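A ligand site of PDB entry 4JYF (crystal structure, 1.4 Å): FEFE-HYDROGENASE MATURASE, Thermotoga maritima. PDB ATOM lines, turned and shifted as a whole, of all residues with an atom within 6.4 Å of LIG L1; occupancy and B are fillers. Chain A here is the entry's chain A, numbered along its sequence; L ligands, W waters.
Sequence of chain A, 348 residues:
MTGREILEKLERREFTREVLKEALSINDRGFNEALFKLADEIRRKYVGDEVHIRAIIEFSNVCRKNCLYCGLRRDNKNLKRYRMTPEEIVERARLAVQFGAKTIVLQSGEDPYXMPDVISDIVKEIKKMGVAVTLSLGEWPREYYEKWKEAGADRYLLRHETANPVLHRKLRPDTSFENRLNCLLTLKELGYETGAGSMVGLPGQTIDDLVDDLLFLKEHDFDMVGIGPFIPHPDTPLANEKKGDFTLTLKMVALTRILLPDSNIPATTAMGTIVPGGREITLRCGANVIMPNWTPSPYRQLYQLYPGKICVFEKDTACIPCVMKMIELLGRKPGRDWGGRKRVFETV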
ATOM      1  N   VAL A  62     -19.182   4.026 -20.193  1.00  0.00           N
ATOM      2  CA  VAL A  62     -19.155   2.843 -21.051  1.00  0.00           C
ATOM      3  C   VAL A  62     -19.710   3.211 -22.421  1.00  0.00           C
ATOM      4  O   VAL A  62     -20.727   3.885 -22.512  1.00  0.00           O
ATOM      5  CB  VAL A  62     -19.951   1.702 -20.444  1.00  0.00           C
ATOM      6  CG1 VAL A  62     -20.094   0.512 -21.417  1.00  0.00           C
ATOM      7  CG2 VAL A  62     -19.270   1.274 -19.135  1.00  0.00           C
ATOM      8  N   CYS A  63     -19.000   2.839 -23.480  1.00  0.00           N
ATOM      9  CA  CYS A  63     -19.506   3.084 -24.830  1.00  0.00           C
ATOM     10  C   CYS A  63     -19.242   1.949 -25.785  1.00  0.00           C
ATOM     11  O   CYS A  63     -18.131   1.405 -25.808  1.00  0.00           O
ATOM     12  CB  CYS A  63     -18.947   4.384 -25.423  1.00  0.00           C
ATOM     13  SG  CYS A  63     -19.917   4.930 -26.870  1.00  0.00           S
ATOM     14  N   ARG A  64     -20.241   1.674 -26.609  1.00  0.00           N
ATOM     15  CA  ARG A  64     -20.132   0.656 -27.661  1.00  0.00           C
ATOM     16  C   ARG A  64     -19.580   1.184 -28.981  1.00  0.00           C
ATOM     17  O   ARG A  64     -19.203   0.385 -29.850  1.00  0.00           O
ATOM     18  CB  ARG A  64     -21.512   0.072 -27.925  1.00  0.00           C
ATOM     19  CG  ARG A  64     -22.489   1.061 -28.580  1.00  0.00           C
ATOM     20  CD  ARG A  64     -23.866   0.505 -28.680  1.00  0.00           C
ATOM     21  NE  ARG A  64     -24.779   1.478 -29.237  1.00  0.00           N
ATOM     22  CZ  ARG A  64     -25.990   1.207 -29.704  1.00  0.00           C
ATOM     23  NH1 ARG A  64     -26.474  -0.040 -29.745  1.00  0.00           N
ATOM     24  NH2 ARG A  64     -26.717   2.200 -30.192  1.00  0.00           N
ATOM     25  N   LYS A  65     -19.576   2.507 -29.157  1.00  0.00           N
ATOM     26  CA  LYS A  65     -19.098   3.114 -30.398  1.00  0.00           C
ATOM     27  C   LYS A  65     -17.606   3.459 -30.315  1.00  0.00           C
ATOM     28  O   LYS A  65     -16.990   3.377 -29.237  1.00  0.00           O
ATOM     29  CB  LYS A  65     -19.934   4.332 -30.768  1.00  0.00           C
ATOM     30  CG  LYS A  65     -21.272   3.980 -31.411  1.00  0.00           C
ATOM     31  CD  LYS A  65     -22.024   5.189 -31.872  1.00  0.00           C
ATOM     32  CE  LYS A  65     -23.182   4.853 -32.773  1.00  0.00           C
ATOM     33  NZ  LYS A  65     -24.170   3.861 -32.306  1.00  0.00           N
ATOM     34  N   ASN A  66     -17.036   3.844 -31.454  1.00  0.00           N
ATOM     35  CA  ASN A  66     -15.592   3.992 -31.576  1.00  0.00           C
ATOM     36  C   ASN A  66     -15.219   5.308 -32.258  1.00  0.00           C
ATOM     37  O   ASN A  66     -14.237   5.371 -32.990  1.00  0.00           O
ATOM     38  CB  ASN A  66     -14.990   2.799 -32.353  1.00  0.00           C
ATOM     39  CG  ASN A  66     -13.585   2.413 -31.910  1.00  0.00           C
ATOM     40  OD1 ASN A  66     -13.116   2.713 -30.808  1.00  0.00           O
ATOM     41  ND2 ASN A  66     -12.903   1.681 -32.788  1.00  0.00           N
ATOM     42  N   CYS A  67     -15.955   6.372 -31.974  1.00  0.00           N
ATOM     43  CA  CYS A  67     -15.709   7.671 -32.606  1.00  0.00           C
ATOM     44  C   CYS A  67     -14.254   8.058 -32.453  1.00  0.00           C
ATOM     45  O   CYS A  67     -13.677   7.950 -31.397  1.00  0.00           O
ATOM     46  CB  CYS A  67     -16.632   8.741 -32.001  1.00  0.00           C
ATOM     47  SG  CYS A  67     -18.393   8.287 -32.052  1.00  0.00           S
ATOM     48  N   LEU A  68     -13.616   8.490 -33.547  1.00  0.00           N
ATOM     49  CA  LEU A  68     -12.168   8.680 -33.525  1.00  0.00           C
ATOM     50  C   LEU A  68     -11.678   9.800 -32.643  1.00  0.00           C
ATOM     51  O   LEU A  68     -10.523   9.800 -32.225  1.00  0.00           O
ATOM     52  CB  LEU A  68     -11.630   8.916 -34.944  1.00  0.00           C
ATOM     53  CG  LEU A  68     -11.315   7.658 -35.778  1.00  0.00           C
ATOM     54  CD1 LEU A  68     -12.509   6.731 -35.971  1.00  0.00           C
ATOM     55  CD2 LEU A  68     -10.705   8.103 -37.111  1.00  0.00           C
ATOM     56  N   TYR A  69     -12.550  10.762 -32.368  1.00  0.00           N
ATOM     57  CA  TYR A  69     -12.184  11.959 -31.581  1.00  0.00           C
ATOM     58  C   TYR A  69     -12.342  11.770 -30.076  1.00  0.00           C
ATOM     59  O   TYR A  69     -11.810  12.557 -29.286  1.00  0.00           O
ATOM     60  CB  TYR A  69     -13.037  13.154 -32.019  1.00  0.00           C
ATOM     61  CG  TYR A  69     -14.492  12.865 -32.172  1.00  0.00           C
ATOM     62  CD1 TYR A  69     -15.330  12.805 -31.063  1.00  0.00           C
ATOM     63  CD2 TYR A  69     -15.055  12.639 -33.437  1.00  0.00           C
ATOM     64  CE1 TYR A  69     -16.669  12.533 -31.213  1.00  0.00           C
ATOM     65  CE2 TYR A  69     -16.381  12.363 -33.590  1.00  0.00           C
ATOM     66  CZ  TYR A  69     -17.205  12.319 -32.484  1.00  0.00           C
ATOM     67  OH  TYR A  69     -18.528  12.029 -32.699  1.00  0.00           O
ATOM     68  N   CYS A  70     -13.088  10.749 -29.686  1.00  0.00           N
ATOM     69  CA  CYS A  70     -13.595  10.664 -28.315  1.00  0.00           C
ATOM     70  C   CYS A  70     -12.838   9.759 -27.382  1.00  0.00           C
ATOM     71  O   CYS A  70     -12.627   8.579 -27.688  1.00  0.00           O
ATOM     72  CB  CYS A  70     -15.038  10.183 -28.358  1.00  0.00           C
ATOM     73  SG  CYS A  70     -15.890  10.186 -26.753  1.00  0.00           S
ATOM     74  N   GLY A  71     -12.473  10.292 -26.215  1.00  0.00           N
ATOM     75  CA  GLY A  71     -11.781   9.508 -25.226  1.00  0.00           C
ATOM     76  C   GLY A  71     -12.518   8.300 -24.684  1.00  0.00           C
ATOM     77  O   GLY A  71     -11.887   7.401 -24.133  1.00  0.00           O
ATOM     78  N   LEU A  72     -13.844   8.283 -24.806  1.00  0.00           N
ATOM     79  CA  LEU A  72     -14.657   7.150 -24.350  1.00  0.00           C
ATOM     80  C   LEU A  72     -14.827   6.032 -25.398  1.00  0.00           C
ATOM     81  O   LEU A  72     -15.464   5.018 -25.157  1.00  0.00           O
ATOM     82  CB  LEU A  72     -16.056   7.590 -23.890  1.00  0.00           C
ATOM     83  CG  LEU A  72     -16.187   8.698 -22.853  1.00  0.00           C
ATOM     84  CD1 LEU A  72     -17.621   8.710 -22.323  1.00  0.00           C
ATOM     85  CD2 LEU A  72     -15.191   8.680 -21.751  1.00  0.00           C
ATOM     86  N   ARG A  73     -14.238   6.210 -26.573  1.00  0.00           N
ATOM     87  CA  ARG A  73     -14.375   5.220 -27.660  1.00  0.00           C
ATOM     88  C   ARG A  73     -14.000   3.821 -27.162  1.00  0.00           C
ATOM     89  O   ARG A  73     -13.107   3.675 -26.323  1.00  0.00           O
ATOM     90  CB  ARG A  73     -13.498   5.600 -28.840  1.00  0.00           C
ATOM     91  CG  ARG A  73     -11.972   5.623 -28.570  1.00  0.00           C
ATOM     92  CD  ARG A  73     -11.187   6.381 -29.646  1.00  0.00           C
ATOM     93  NE  ARG A  73     -11.558   5.962 -30.997  1.00  0.00           N
ATOM     94  CZ  ARG A  73     -10.965   4.999 -31.700  1.00  0.00           C
ATOM     95  NH1 ARG A  73      -9.927   4.337 -31.203  1.00  0.00           N
ATOM     96  NH2 ARG A  73     -11.397   4.705 -32.924  1.00  0.00           N
ATOM     97  N   ARG A  74     -14.673   2.806 -27.703  1.00  0.00           N
ATOM     98  CA  ARG A  74     -14.530   1.463 -27.130  1.00  0.00           C
ATOM     99  C   ARG A  74     -13.112   0.923 -27.173  1.00  0.00           C
ATOM    100  O   ARG A  74     -12.751   0.137 -26.303  1.00  0.00           O
ATOM    101  CB  ARG A  74     -15.477   0.431 -27.720  1.00  0.00           C
ATOM    102  CG  ARG A  74     -15.342   0.210 -29.169  1.00  0.00           C
ATOM    103  CD  ARG A  74     -16.160  -0.983 -29.666  1.00  0.00           C
ATOM    104  NE  ARG A  74     -15.735  -1.185 -31.038  1.00  0.00           N
ATOM    105  CZ  ARG A  74     -16.305  -0.656 -32.107  1.00  0.00           C
ATOM    106  NH1 ARG A  74     -17.451   0.020 -32.025  1.00  0.00           N
ATOM    107  NH2 ARG A  74     -15.754  -0.844 -33.293  1.00  0.00           N
ATOM    108  N   SER A 108     -24.311  10.062 -21.153  1.00  0.00           N
ATOM    109  CA  SER A 108     -23.452   8.881 -21.045  1.00  0.00           C
ATOM    110  C   SER A 108     -22.803   8.553 -22.378  1.00  0.00           C
ATOM    111  O   SER A 108     -23.215   9.039 -23.432  1.00  0.00           O
ATOM    112  CB  SER A 108     -24.252   7.671 -20.540  1.00  0.00           C
ATOM    113  OG  SER A 108     -25.313   7.354 -21.422  1.00  0.00           O
ATOM    114  N   GLY A 109     -21.821   7.649 -22.309  1.00  0.00           N
ATOM    115  CA  GLY A 109     -21.463   6.861 -23.481  1.00  0.00           C
ATOM    116  C   GLY A 109     -22.684   6.067 -23.914  1.00  0.00           C
ATOM    117  O   GLY A 109     -23.697   5.991 -23.196  1.00  0.00           O
ATOM    118  N   GLU A 110     -22.625   5.501 -25.109  1.00  0.00           N
ATOM    119  CA  GLU A 110     -23.668   4.588 -25.543  1.00  0.00           C
ATOM    120  C   GLU A 110     -23.485   3.258 -24.816  1.00  0.00           C
ATOM    121  O   GLU A 110     -22.918   2.298 -25.338  1.00  0.00           O
ATOM    122  CB  GLU A 110     -23.645   4.424 -27.068  1.00  0.00           C
ATOM    123  CG  GLU A 110     -24.130   5.659 -27.828  1.00  0.00           C
ATOM    124  CD  GLU A 110     -24.494   5.387 -29.294  1.00  0.00           C
ATOM    125  OE1 GLU A 110     -24.502   4.197 -29.692  1.00  0.00           O
ATOM    126  OE2 GLU A 110     -24.776   6.358 -30.039  1.00  0.00           O
ATOM    127  N   GLY A 138     -26.913   9.348 -27.005  1.00  0.00           N
ATOM    128  CA  GLY A 138     -26.494   8.888 -28.335  1.00  0.00           C
ATOM    129  C   GLY A 138     -27.665   8.329 -29.150  1.00  0.00           C
ATOM    130  O   GLY A 138     -28.848   8.681 -28.946  1.00  0.00           O
ATOM    131  N   GLU A 161     -22.516  16.798 -35.066  1.00  0.00           N
ATOM    132  CA  GLU A 161     -21.042  16.642 -35.081  1.00  0.00           C
ATOM    133  C   GLU A 161     -20.388  17.309 -36.271  1.00  0.00           C
ATOM    134  O   GLU A 161     -19.519  18.151 -36.094  1.00  0.00           O
ATOM    135  CB  GLU A 161     -20.592  15.182 -34.960  1.00  0.00           C
ATOM    136  CG  GLU A 161     -21.312  14.409 -33.878  1.00  0.00           C
ATOM    137  CD  GLU A 161     -21.081  14.901 -32.453  1.00  0.00           C
ATOM    138  OE1 GLU A 161     -20.417  15.945 -32.228  1.00  0.00           O
ATOM    139  OE2 GLU A 161     -21.579  14.198 -31.536  1.00  0.00           O
ATOM    140  N   ARG A 172     -16.890   8.636 -37.363  1.00  0.00           N
ATOM    141  CA  ARG A 172     -17.884   7.907 -36.597  1.00  0.00           C
ATOM    142  C   ARG A 172     -18.190   6.623 -37.347  1.00  0.00           C
ATOM    143  O   ARG A 172     -19.268   6.466 -37.937  1.00  0.00           O
ATOM    144  CB  ARG A 172     -19.109   8.785 -36.362  1.00  0.00           C
ATOM    145  CG  ARG A 172     -18.744  10.158 -35.811  1.00  0.00           C
ATOM    146  CD  ARG A 172     -19.933  10.978 -35.390  1.00  0.00           C
ATOM    147  NE  ARG A 172     -20.509  10.334 -34.208  1.00  0.00           N
ATOM    148  CZ  ARG A 172     -21.684   9.749 -34.129  1.00  0.00           C
ATOM    149  NH1 ARG A 172     -22.530   9.801 -35.144  1.00  0.00           N
ATOM    150  NH2 ARG A 172     -22.013   9.076 -33.005  1.00  0.00           N
ATOM    151  N   ARG A 180     -27.660   9.886 -38.116  1.00  0.00           N
ATOM    152  CA  ARG A 180     -27.680  10.958 -37.105  1.00  0.00           C
ATOM    153  C   ARG A 180     -28.847  11.923 -37.367  1.00  0.00           C
ATOM    154  O   ARG A 180     -29.626  12.247 -36.456  1.00  0.00           O
ATOM    155  CB  ARG A 180     -26.342  11.694 -37.109  1.00  0.00           C
ATOM    156  CG  ARG A 180     -26.032  12.503 -35.877  1.00  0.00           C
ATOM    157  CD  ARG A 180     -25.683  11.627 -34.706  1.00  0.00           C
ATOM    158  NE  ARG A 180     -25.172  12.382 -33.583  1.00  0.00           N
ATOM    159  CZ  ARG A 180     -24.778  11.835 -32.442  1.00  0.00           C
ATOM    160  NH1 ARG A 180     -24.861  10.520 -32.248  1.00  0.00           N
ATOM    161  NH2 ARG A 180     -24.338  12.596 -31.467  1.00  0.00           N
ATOM    162  N   TYR A 303     -14.778  10.690 -16.898  1.00  0.00           N
ATOM    163  CA  TYR A 303     -15.602  11.031 -18.071  1.00  0.00           C
ATOM    164  C   TYR A 303     -14.811  12.018 -18.913  1.00  0.00           C
ATOM    165  O   TYR A 303     -15.010  13.227 -18.836  1.00  0.00           O
ATOM    166  CB  TYR A 303     -16.937  11.579 -17.657  1.00  0.00           C
ATOM    167  CG  TYR A 303     -17.946  11.616 -18.777  1.00  0.00           C
ATOM    168  CD1 TYR A 303     -18.713  10.490 -19.070  1.00  0.00           C
ATOM    169  CD2 TYR A 303     -18.140  12.758 -19.533  1.00  0.00           C
ATOM    170  CE1 TYR A 303     -19.654  10.511 -20.073  1.00  0.00           C
ATOM    171  CE2 TYR A 303     -19.078  12.801 -20.526  1.00  0.00           C
ATOM    172  CZ  TYR A 303     -19.836  11.666 -20.801  1.00  0.00           C
ATOM    173  OH  TYR A 303     -20.785  11.706 -21.801  1.00  0.00           O
ATOM    174  N   LEU A 305     -14.079  12.865 -22.401  1.00  0.00           N
ATOM    175  CA  LEU A 305     -14.299  12.927 -23.848  1.00  0.00           C
ATOM    176  C   LEU A 305     -13.045  13.526 -24.480  1.00  0.00           C
ATOM    177  O   LEU A 305     -12.597  13.093 -25.529  1.00  0.00           O
ATOM    178  CB  LEU A 305     -15.521  13.795 -24.149  1.00  0.00           C
ATOM    179  CG  LEU A 305     -16.871  13.398 -23.536  1.00  0.00           C
ATOM    180  CD1 LEU A 305     -17.877  14.562 -23.774  1.00  0.00           C
ATOM    181  CD2 LEU A 305     -17.364  12.088 -24.078  1.00  0.00           C
HETATM  182 FE1  LIG L   1     -18.952   8.472 -29.796  1.00  0.00          FE
HETATM  183 FE2  LIG L   1     -20.618   9.544 -27.744  1.00  0.00          FE
HETATM  184 FE3  LIG L   1     -19.291   7.010 -27.520  1.00  0.00          FE
HETATM  185 FE4  LIG L   1     -17.808   9.244 -27.424  1.00  0.00          FE
HETATM  186  S1  LIG L   1     -19.374   8.686 -25.930  1.00  0.00           S
HETATM  187  S2  LIG L   1     -17.347   7.297 -28.600  1.00  0.00           S
HETATM  188  S3  LIG L   1     -18.940  10.621 -28.896  1.00  0.00           S
HETATM  189  S4  LIG L   1     -20.915   7.623 -29.082  1.00  0.00           S
HETATM  190  N1  LG2 L   2     -22.438   9.468 -26.488  1.00  0.00           N
HETATM  191  C1  LG2 L   2     -23.376  10.612 -26.670  1.00  0.00           C
HETATM  192  C2  LG2 L   2     -23.127  11.673 -25.588  1.00  0.00           C
HETATM  193  C3  LG2 L   2     -21.730  11.914 -25.103  1.00  0.00           C
HETATM  194  S1  LG2 L   2     -20.644  12.630 -26.322  1.00  0.00           S
HETATM  195  C4  LG2 L   2     -23.231  11.147 -28.080  1.00  0.00           C
HETATM  196  O1  LG2 L   2     -22.246  10.767 -28.751  1.00  0.00           O
HETATM  197  O2  LG2 L   2     -24.041  11.960 -28.558  1.00  0.00           O
HETATM  198  C5  LG2 L   2     -21.067  14.401 -26.049  1.00  0.00           C
HETATM  199  C6  LG2 L   2     -20.434  15.371 -27.069  1.00  0.00           C
HETATM  200  O3  LG2 L   2     -19.075  15.666 -26.739  1.00  0.00           O
HETATM  201  C7  LG2 L   2     -20.355  14.906 -28.515  1.00  0.00           C
HETATM  202  O4  LG2 L   2     -21.559  15.111 -29.220  1.00  0.00           O
HETATM  203  C8  LG2 L   2     -19.165  15.659 -29.111  1.00  0.00           C
HETATM  204  O5  LG2 L   2     -19.506  16.785 -29.904  1.00  0.00           O
HETATM  205  C9  LG2 L   2     -18.344  16.098 -27.865  1.00  0.00           C
HETATM  206  N2  LG2 L   2     -16.962  15.574 -27.890  1.00  0.00           N
HETATM  207  C10 LG2 L   2     -16.586  14.260 -27.895  1.00  0.00           C
HETATM  208  N3  LG2 L   2     -15.249  14.171 -27.981  1.00  0.00           N
HETATM  209  C11 LG2 L   2     -14.757  15.438 -28.106  1.00  0.00           C
HETATM  210  C12 LG2 L   2     -13.480  15.960 -28.209  1.00  0.00           C
HETATM  211  N4  LG2 L   2     -12.391  15.196 -28.319  1.00  0.00           N
HETATM  212  N5  LG2 L   2     -13.315  17.331 -28.278  1.00  0.00           N
HETATM  213  C13 LG2 L   2     -14.368  18.191 -28.207  1.00  0.00           C
HETATM  214  N6  LG2 L   2     -15.627  17.673 -28.068  1.00  0.00           N
HETATM  215  C14 LG2 L   2     -15.832  16.330 -28.020  1.00  0.00           C
HETATM  216  O   HOH W   1     -20.906  11.561 -31.374  1.00  0.00           O
HETATM  217  O   HOH W   2     -23.762   8.805 -30.379  1.00  0.00           O
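The guanidinium group (NH2) of Arg 180 is in salt-bridge range of an oxygen (O2) of LG2 L2 (3.0 Å).
The side-chain sulfur of Cys 70 is bound to an iron atom (FE4) of LIG L1 (2.2 Å).
S2 of LIG L1 sits close to N of Cys 67 (3.8 Å).
An iron atom (FE1) of LIG L1 is bound by the side-chain sulfur (SG) of Cys 67 (2.3 Å).
The side-chain sulfur (SG) of Cys 63 is bound to an iron atom (FE3) of LIG L1 (2.3 Å).
The backbone carbonyl oxygen (O) of Ser 108 sits close to a nitrogen (N1) of LG2 L2.
OE2 of Glu 161 is in hydrogen-bond range of O4 of LG2 L2, 2.5 Å away.
N4 of LG2 L2 sits at hydrogen-bond distance from O of Tyr 69, 2.9 Å away.
The backbone carbonyl oxygen (O) of Leu 305 is in hydrogen-bond range of a nitrogen (N4) of LG2 L2 (3.5 Å).
N1 of LG2 L2 binds FE2 of LIG L1.
The backbone carbonyl oxygen (O) of Asn 66 sits at hydrogen-bond distance from the guanidinium group (NH2) of Arg 73.
The guanidinium group (NE) of Arg 172 lies within hydrogen-bond range of the side-chain hydroxyl (OH) of Tyr 69, at 3.0 Å.
The side-chain sulfur (SG) of Cys 63 lies close to the backbone NH (N) of Lys 65.
The backbone NH (N) of Glu 110 sits close to the side-chain sulfur (SG) of Cys 63 (3.3 Å).
N of Arg 74 is in hydrogen-bond range of O of Lys 65 (2.8 Å).
The guanidinium group (NE) of Arg 172 lies close to the side-chain sulfur (SG) of Cys 67 (3.6 Å).
The side-chain sulfur (SG) of Cys 70 lies close to the backbone NH (N) of Leu 72.
The side-chain sulfur of Cys 67 sits close to the side-chain hydroxyl of Tyr 69 (3.8 Å).
CB of Lys 65 touches S4 of LIG L1 (3.8 Å).
CE1 of Tyr 69 touches S3 of LIG L1, 3.8 Å away.
Arg 73 touches LIG L1 (CA to S2, 3.7 Å).
CA of Gly 109 touches S1 of LIG L1, at 3.7 Å.
Glu 110 touches LIG L1 (CG to S4, 3.97 Å).
Hydrophobic or aromatic side chains within 4 Å of LIG L1: Tyr 69.
Eight residues have an atom within 4 Å of LIG L1: Cys 63, Lys 65, Cys 67, Tyr 69, Cys 70, Arg 73, Gly 109 and Glu 110.
The nearest printed residue that does not touch LIG L1 is Leu 72 (4.01 Å).
Water W1 lies within hydrogen-bond range of OE2 of Glu 161 (2.7 Å), OH of Tyr 69 (2.8 Å), NE of Arg 172 (3.1 Å) and S3 of LIG L1 (3.3 Å).
Water W2 lies within hydrogen-bond range of OE2 of Glu 110 (2.7 Å), NH1 of Arg 180 (2.8 Å), NH2 of Arg 172 (3.2 Å) and S4 of LIG L1 (3.3 Å).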
